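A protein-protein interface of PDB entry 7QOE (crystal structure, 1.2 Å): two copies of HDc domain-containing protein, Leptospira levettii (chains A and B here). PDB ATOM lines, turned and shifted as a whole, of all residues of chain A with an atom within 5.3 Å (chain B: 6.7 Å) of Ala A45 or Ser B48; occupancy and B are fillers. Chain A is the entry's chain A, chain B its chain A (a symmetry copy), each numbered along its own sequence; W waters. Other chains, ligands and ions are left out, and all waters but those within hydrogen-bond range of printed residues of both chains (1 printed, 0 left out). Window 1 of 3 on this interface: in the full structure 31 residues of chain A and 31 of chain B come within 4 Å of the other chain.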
ATOM      1  N   ILE A  40      18.512  -0.877  15.212  1.00  0.00           N
ATOM      2  CA  ILE A  40      18.286  -2.319  15.169  1.00  0.00           C
ATOM      3  C   ILE A  40      16.867  -2.672  15.579  1.00  0.00           C
ATOM      4  O   ILE A  40      16.329  -3.690  15.130  1.00  0.00           O
ATOM      5  CB  ILE A  40      19.364  -3.049  16.008  1.00  0.00           C
ATOM      6  CG1 ILE A  40      19.324  -4.574  15.801  1.00  0.00           C
ATOM      7  CG2 ILE A  40      19.235  -2.716  17.509  1.00  0.00           C
ATOM      8  CD1 ILE A  40      19.470  -5.062  14.358  1.00  0.00           C
ATOM      9  N   THR A  41      16.217  -1.849  16.402  1.00  0.00           N
ATOM     10  CA  THR A  41      14.842  -2.143  16.792  1.00  0.00           C
ATOM     11  C   THR A  41      13.935  -2.259  15.567  1.00  0.00           C
ATOM     12  O   THR A  41      13.018  -3.087  15.548  1.00  0.00           O
ATOM     13  CB  THR A  41      14.287  -1.078  17.748  1.00  0.00           C
ATOM     14  OG1 THR A  41      14.356   0.218  17.150  1.00  0.00           O
ATOM     15  CG2 THR A  41      15.065  -1.058  19.069  1.00  0.00           C
ATOM     16  N   HIS A  42      14.136  -1.393  14.567  1.00  0.00           N
ATOM     17  CA  HIS A  42      13.314  -1.432  13.358  1.00  0.00           C
ATOM     18  C   HIS A  42      13.551  -2.728  12.600  1.00  0.00           C
ATOM     19  O   HIS A  42      12.606  -3.366  12.123  1.00  0.00           O
ATOM     20  CB  HIS A  42      13.611  -0.196  12.480  1.00  0.00           C
ATOM     21  CG  HIS A  42      13.159  -0.323  11.050  1.00  0.00           C
ATOM     22  ND1 HIS A  42      11.828  -0.296  10.690  1.00  0.00           N
ATOM     23  CD2 HIS A  42      13.861  -0.334   9.889  1.00  0.00           C
ATOM     24  CE1 HIS A  42      11.729  -0.358   9.372  1.00  0.00           C
ATOM     25  NE2 HIS A  42      12.949  -0.373   8.863  1.00  0.00           N
ATOM     26  N   LEU A  43      14.816  -3.110  12.442  1.00  0.00           N
ATOM     27  CA  LEU A  43      15.165  -4.296  11.675  1.00  0.00           C
ATOM     28  C   LEU A  43      14.648  -5.565  12.334  1.00  0.00           C
ATOM     29  O   LEU A  43      14.139  -6.461  11.641  1.00  0.00           O
ATOM     30  CB  LEU A  43      16.678  -4.321  11.488  1.00  0.00           C
ATOM     31  CG  LEU A  43      17.270  -3.088  10.788  1.00  0.00           C
ATOM     32  CD1 LEU A  43      18.801  -3.119  10.716  1.00  0.00           C
ATOM     33  CD2 LEU A  43      16.644  -2.899   9.396  1.00  0.00           C
ATOM     34  N   LEU A  44      14.718  -5.647  13.664  1.00  0.00           N
ATOM     35  CA  LEU A  44      14.176  -6.803  14.369  1.00  0.00           C
ATOM     36  C   LEU A  44      12.669  -6.879  14.191  1.00  0.00           C
ATOM     37  O   LEU A  44      12.112  -7.967  13.990  1.00  0.00           O
ATOM     38  CB  LEU A  44      14.506  -6.735  15.862  1.00  0.00           C
ATOM     39  CG  LEU A  44      15.989  -6.811  16.224  1.00  0.00           C
ATOM     40  CD1 LEU A  44      16.096  -6.894  17.751  1.00  0.00           C
ATOM     41  CD2 LEU A  44      16.710  -7.974  15.573  1.00  0.00           C
ATOM     42  N   ALA A  45      11.989  -5.735  14.254  1.00  0.00           N
ATOM     43  CA  ALA A  45      10.541  -5.701  14.098  1.00  0.00           C
ATOM     44  C   ALA A  45      10.127  -6.159  12.703  1.00  0.00           C
ATOM     45  O   ALA A  45       9.176  -6.938  12.551  1.00  0.00           O
ATOM     46  CB  ALA A  45      10.015  -4.284  14.358  1.00  0.00           C
ATOM     47  N   VAL A  46      10.838  -5.694  11.675  1.00  0.00           N
ATOM     48  CA  VAL A  46      10.523  -6.078  10.299  1.00  0.00           C
ATOM     49  C   VAL A  46      10.774  -7.561  10.095  1.00  0.00           C
ATOM     50  O   VAL A  46       9.950  -8.262   9.489  1.00  0.00           O
ATOM     51  CB  VAL A  46      11.340  -5.198   9.339  1.00  0.00           C
ATOM     52  CG1 VAL A  46      11.264  -5.730   7.915  1.00  0.00           C
ATOM     53  CG2 VAL A  46      10.863  -3.749   9.404  1.00  0.00           C
ATOM     54  N   ALA A  47      11.896  -8.076  10.597  1.00  0.00           N
ATOM     55  CA  ALA A  47      12.172  -9.508  10.497  1.00  0.00           C
ATOM     56  C   ALA A  47      11.082 -10.325  11.178  1.00  0.00           C
ATOM     57  O   ALA A  47      10.635 -11.350  10.642  1.00  0.00           O
ATOM     58  CB  ALA A  47      13.538  -9.829  11.110  1.00  0.00           C
ATOM     59  N   SER A  48      10.633  -9.885  12.356  1.00  0.00           N
ATOM     60  CA  SER A  48       9.547 -10.554  13.061  1.00  0.00           C
ATOM     61  C   SER A  48       8.282 -10.601  12.217  1.00  0.00           C
ATOM     62  O   SER A  48       7.652 -11.658  12.098  1.00  0.00           O
ATOM     63  CB  SER A  48       9.278  -9.841  14.392  1.00  0.00           C
ATOM     64  OG  SER A  48       8.194 -10.453  15.067  1.00  0.00           O
ATOM     65  N   ILE A  49       7.878  -9.461  11.650  1.00  0.00           N
ATOM     66  CA  ILE A  49       6.663  -9.411  10.841  1.00  0.00           C
ATOM     67  C   ILE A  49       6.774 -10.363   9.654  1.00  0.00           C
ATOM     68  O   ILE A  49       5.840 -11.118   9.352  1.00  0.00           O
ATOM     69  CB  ILE A  49       6.392  -7.962  10.382  1.00  0.00           C
ATOM     70  CG1 ILE A  49       6.007  -7.052  11.553  1.00  0.00           C
ATOM     71  CG2 ILE A  49       5.304  -7.919   9.308  1.00  0.00           C
ATOM     72  CD1 ILE A  49       6.209  -5.583  11.246  1.00  0.00           C
ATOM     73  N   ILE A  50       7.919 -10.356   8.971  1.00  0.00           N
ATOM     74  CA  ILE A  50       8.103 -11.237   7.819  1.00  0.00           C
ATOM     75  C   ILE A  50       7.968 -12.688   8.256  1.00  0.00           C
ATOM     76  O   ILE A  50       7.300 -13.493   7.593  1.00  0.00           O
ATOM     77  CB  ILE A  50       9.474 -10.975   7.178  1.00  0.00           C
ATOM     78  CG1 ILE A  50       9.484  -9.589   6.531  1.00  0.00           C
ATOM     79  CG2 ILE A  50       9.806 -12.060   6.129  1.00  0.00           C
ATOM     80  CD1 ILE A  50      10.861  -9.055   6.273  1.00  0.00           C
ATOM     81  N   HIS A 136       5.822  -1.521   9.851  1.00  0.00           N
ATOM     82  CA  HIS A 136       6.513  -1.105  11.064  1.00  0.00           C
ATOM     83  C   HIS A 136       6.638   0.413  11.133  1.00  0.00           C
ATOM     84  O   HIS A 136       6.448   1.016  12.198  1.00  0.00           O
ATOM     85  CB  HIS A 136       7.880  -1.745  11.176  1.00  0.00           C
ATOM     86  CG  HIS A 136       8.558  -1.367  12.450  1.00  0.00           C
ATOM     87  ND1 HIS A 136       9.663  -0.552  12.500  1.00  0.00           N
ATOM     88  CD2 HIS A 136       8.203  -1.600  13.734  1.00  0.00           C
ATOM     89  CE1 HIS A 136       9.996  -0.347  13.759  1.00  0.00           C
ATOM     90  NE2 HIS A 136       9.124  -0.970  14.527  1.00  0.00           N
ATOM     91  N   LEU B  43      10.072 -13.138  20.326  1.00  0.00           N
ATOM     92  CA  LEU B  43      11.147 -12.590  21.140  1.00  0.00           C
ATOM     93  C   LEU B  43      11.785 -11.375  20.484  1.00  0.00           C
ATOM     94  O   LEU B  43      12.078 -10.382  21.170  1.00  0.00           O
ATOM     95  CB  LEU B  43      12.161 -13.697  21.408  1.00  0.00           C
ATOM     96  CG  LEU B  43      11.598 -14.942  22.109  1.00  0.00           C
ATOM     97  CD1 LEU B  43      12.634 -16.061  22.262  1.00  0.00           C
ATOM     98  CD2 LEU B  43      10.967 -14.569  23.460  1.00  0.00           C
ATOM     99  N   LEU B  44      11.964 -11.404  19.162  1.00  0.00           N
ATOM    100  CA  LEU B  44      12.503 -10.246  18.457  1.00  0.00           C
ATOM    101  C   LEU B  44      11.549  -9.069  18.556  1.00  0.00           C
ATOM    102  O   LEU B  44      11.979  -7.924  18.753  1.00  0.00           O
ATOM    103  CB  LEU B  44      12.751 -10.574  16.983  1.00  0.00           C
ATOM    104  CG  LEU B  44      13.812 -11.638  16.702  1.00  0.00           C
ATOM    105  CD1 LEU B  44      14.026 -11.698  15.186  1.00  0.00           C
ATOM    106  CD2 LEU B  44      15.123 -11.385  17.419  1.00  0.00           C
ATOM    107  N   ALA B  45      10.247  -9.326  18.430  1.00  0.00           N
ATOM    108  CA  ALA B  45       9.251  -8.265  18.508  1.00  0.00           C
ATOM    109  C   ALA B  45       9.243  -7.617  19.889  1.00  0.00           C
ATOM    110  O   ALA B  45       9.184  -6.386  20.008  1.00  0.00           O
ATOM    111  CB  ALA B  45       7.860  -8.823  18.186  1.00  0.00           C
ATOM    112  N   VAL B  46       9.315  -8.433  20.942  1.00  0.00           N
ATOM    113  CA  VAL B  46       9.318  -7.910  22.308  1.00  0.00           C
ATOM    114  C   VAL B  46      10.580  -7.104  22.560  1.00  0.00           C
ATOM    115  O   VAL B  46      10.522  -6.008  23.138  1.00  0.00           O
ATOM    116  CB  VAL B  46       9.153  -9.082  23.288  1.00  0.00           C
ATOM    117  CG1 VAL B  46       9.423  -8.636  24.719  1.00  0.00           C
ATOM    118  CG2 VAL B  46       7.760  -9.693  23.164  1.00  0.00           C
ATOM    119  N   ALA B  47      11.735  -7.609  22.132  1.00  0.00           N
ATOM    120  CA  ALA B  47      12.981  -6.859  22.280  1.00  0.00           C
ATOM    121  C   ALA B  47      12.902  -5.518  21.562  1.00  0.00           C
ATOM    122  O   ALA B  47      13.340  -4.490  22.098  1.00  0.00           O
ATOM    123  CB  ALA B  47      14.161  -7.678  21.749  1.00  0.00           C
ATOM    124  N   SER B  48      12.339  -5.505  20.351  1.00  0.00           N
ATOM    125  CA  SER B  48      12.153  -4.266  19.606  1.00  0.00           C
ATOM    126  C   SER B  48      11.303  -3.272  20.382  1.00  0.00           C
ATOM    127  O   SER B  48      11.666  -2.095  20.492  1.00  0.00           O
ATOM    128  CB  SER B  48      11.514  -4.573  18.245  1.00  0.00           C
ATOM    129  OG  SER B  48      11.286  -3.373  17.528  1.00  0.00           O
ATOM    130  N   ILE B  49      10.154  -3.717  20.899  1.00  0.00           N
ATOM    131  CA  ILE B  49       9.267  -2.825  21.641  1.00  0.00           C
ATOM    132  C   ILE B  49       9.987  -2.245  22.854  1.00  0.00           C
ATOM    133  O   ILE B  49       9.913  -1.039  23.124  1.00  0.00           O
ATOM    134  CB  ILE B  49       7.982  -3.578  22.050  1.00  0.00           C
ATOM    135  CG1 ILE B  49       7.111  -3.925  20.838  1.00  0.00           C
ATOM    136  CG2 ILE B  49       7.170  -2.769  23.063  1.00  0.00           C
ATOM    137  CD1 ILE B  49       6.133  -5.046  21.120  1.00  0.00           C
ATOM    138  N   ILE B  50      10.706  -3.086  23.597  1.00  0.00           N
ATOM    139  CA  ILE B  50      11.424  -2.610  24.778  1.00  0.00           C
ATOM    140  C   ILE B  50      12.439  -1.553  24.370  1.00  0.00           C
ATOM    141  O   ILE B  50      12.560  -0.503  25.015  1.00  0.00           O
ATOM    142  CB  ILE B  50      12.105  -3.791  25.485  1.00  0.00           C
ATOM    143  CG1 ILE B  50      11.044  -4.706  26.098  1.00  0.00           C
ATOM    144  CG2 ILE B  50      13.078  -3.291  26.576  1.00  0.00           C
ATOM    145  CD1 ILE B  50      11.547  -6.083  26.417  1.00  0.00           C
ATOM    146  N   GLY B  51      13.205  -1.813  23.312  1.00  0.00           N
ATOM    147  CA  GLY B  51      14.160  -0.824  22.840  1.00  0.00           C
ATOM    148  C   GLY B  51      13.510   0.487  22.443  1.00  0.00           C
ATOM    149  O   GLY B  51      14.034   1.567  22.738  1.00  0.00           O
ATOM    150  N   GLU B  52      12.358   0.415  21.780  1.00  0.00           N
ATOM    151  CA  GLU B  52      11.646   1.616  21.361  1.00  0.00           C
ATOM    152  C   GLU B  52      11.117   2.430  22.534  1.00  0.00           C
ATOM    153  O   GLU B  52      10.867   3.631  22.372  1.00  0.00           O
ATOM    154  CB  GLU B  52      10.489   1.220  20.440  1.00  0.00           C
ATOM    155  CG  GLU B  52      10.940   0.831  19.054  1.00  0.00           C
ATOM    156  CD  GLU B  52       9.812   0.318  18.188  1.00  0.00           C
ATOM    157  OE1 GLU B  52       8.738  -0.027  18.730  1.00  0.00           O
ATOM    158  OE2 GLU B  52      10.000   0.256  16.964  1.00  0.00           O
ATOM    159  N   CYS B  53      10.924   1.808  23.688  1.00  0.00           N
ATOM    160  CA  CYS B  53      10.543   2.501  24.916  1.00  0.00           C
ATOM    161  C   CYS B  53      11.739   3.019  25.694  1.00  0.00           C
ATOM    162  O   CYS B  53      11.577   3.459  26.843  1.00  0.00           O
ATOM    163  CB  CYS B  53       9.739   1.560  25.807  1.00  0.00           C
ATOM    164  SG  CYS B  53       8.153   1.117  25.137  1.00  0.00           S
ATOM    165  N   VAL B  60      16.458  -5.020  27.228  1.00  0.00           N
ATOM    166  CA  VAL B  60      16.222  -5.614  25.910  1.00  0.00           C
ATOM    167  C   VAL B  60      16.623  -7.079  25.924  1.00  0.00           C
ATOM    168  O   VAL B  60      15.910  -7.935  25.375  1.00  0.00           O
ATOM    169  CB  VAL B  60      16.982  -4.806  24.844  1.00  0.00           C
ATOM    170  CG1 VAL B  60      16.925  -5.527  23.509  1.00  0.00           C
ATOM    171  CG2 VAL B  60      16.398  -3.409  24.695  1.00  0.00           C
ATOM    172  N   LEU B  64      14.422 -10.526  25.154  1.00  0.00           N
ATOM    173  CA  LEU B  64      14.731 -11.667  24.301  1.00  0.00           C
ATOM    174  C   LEU B  64      14.606 -12.985  25.047  1.00  0.00           C
ATOM    175  O   LEU B  64      14.265 -14.010  24.440  1.00  0.00           O
ATOM    176  CB  LEU B  64      16.151 -11.541  23.774  1.00  0.00           C
ATOM    177  CG  LEU B  64      16.413 -10.452  22.738  1.00  0.00           C
ATOM    178  CD1 LEU B  64      17.915 -10.288  22.538  1.00  0.00           C
ATOM    179  CD2 LEU B  64      15.739 -10.793  21.409  1.00  0.00           C
HETATM  180  O   HOH W   1       6.955   0.675  16.398  1.00  0.00           O
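Hydrophobic or aromatic side chains of chain B within 4 Å of the printed part of chain A: Ala B45.
Among the printed residues, 6 pairs touch across the chains.
Ala A45 touches Ser B48, and with the chains exchanged Ser A48 touches Ala B45.
Of the 6 pairs that touch across the chains among the printed residues, 2 have their exchanged pair printed and touching as well.
Among the printed residues, merely in contact across the chains: Thr A41 with Gly B51 (3.9 Å), Thr A41 with Glu B52 (3.96 Å), Ala A45 with Ser B48 (3.5 Å) and Ser A48 with Ala B45 (3.5 Å).
Water W1 bridges the side-chain carboxylate of Glu B52 and a ring nitrogen (NE2) of His A136.
NE2 of His A136 is in hydrogen-bond range of OE2 of Glu B52, at 2.9 Å.
The backbone carbonyl oxygen (O) of Thr A41 lies within hydrogen-bond range of the side-chain hydroxyl (OG) of Ser B48, 2.6 Å away.
ND1 of His A136 lies within hydrogen-bond range of ND1 of His A42 (2.8 Å).
Ser B48 touches just these residues of chain A: Thr A41 and Ala A45.
Of the printed residues of chain B, Ser A48 touches Ala B45.
Printed residues of chain B within 4 Å of Thr A41: Ser B48, Gly B51 and Glu B52.
The nearest residue of chain B that does not touch Ala A45 is Leu B44 (5.0 Å).
The nearest printed residue of chain A that does not touch Ser B48 is Leu A44 (4.4 Å).
The nearest printed residue of chain A that does not touch Glu B52 is His A42 (5.1 Å).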
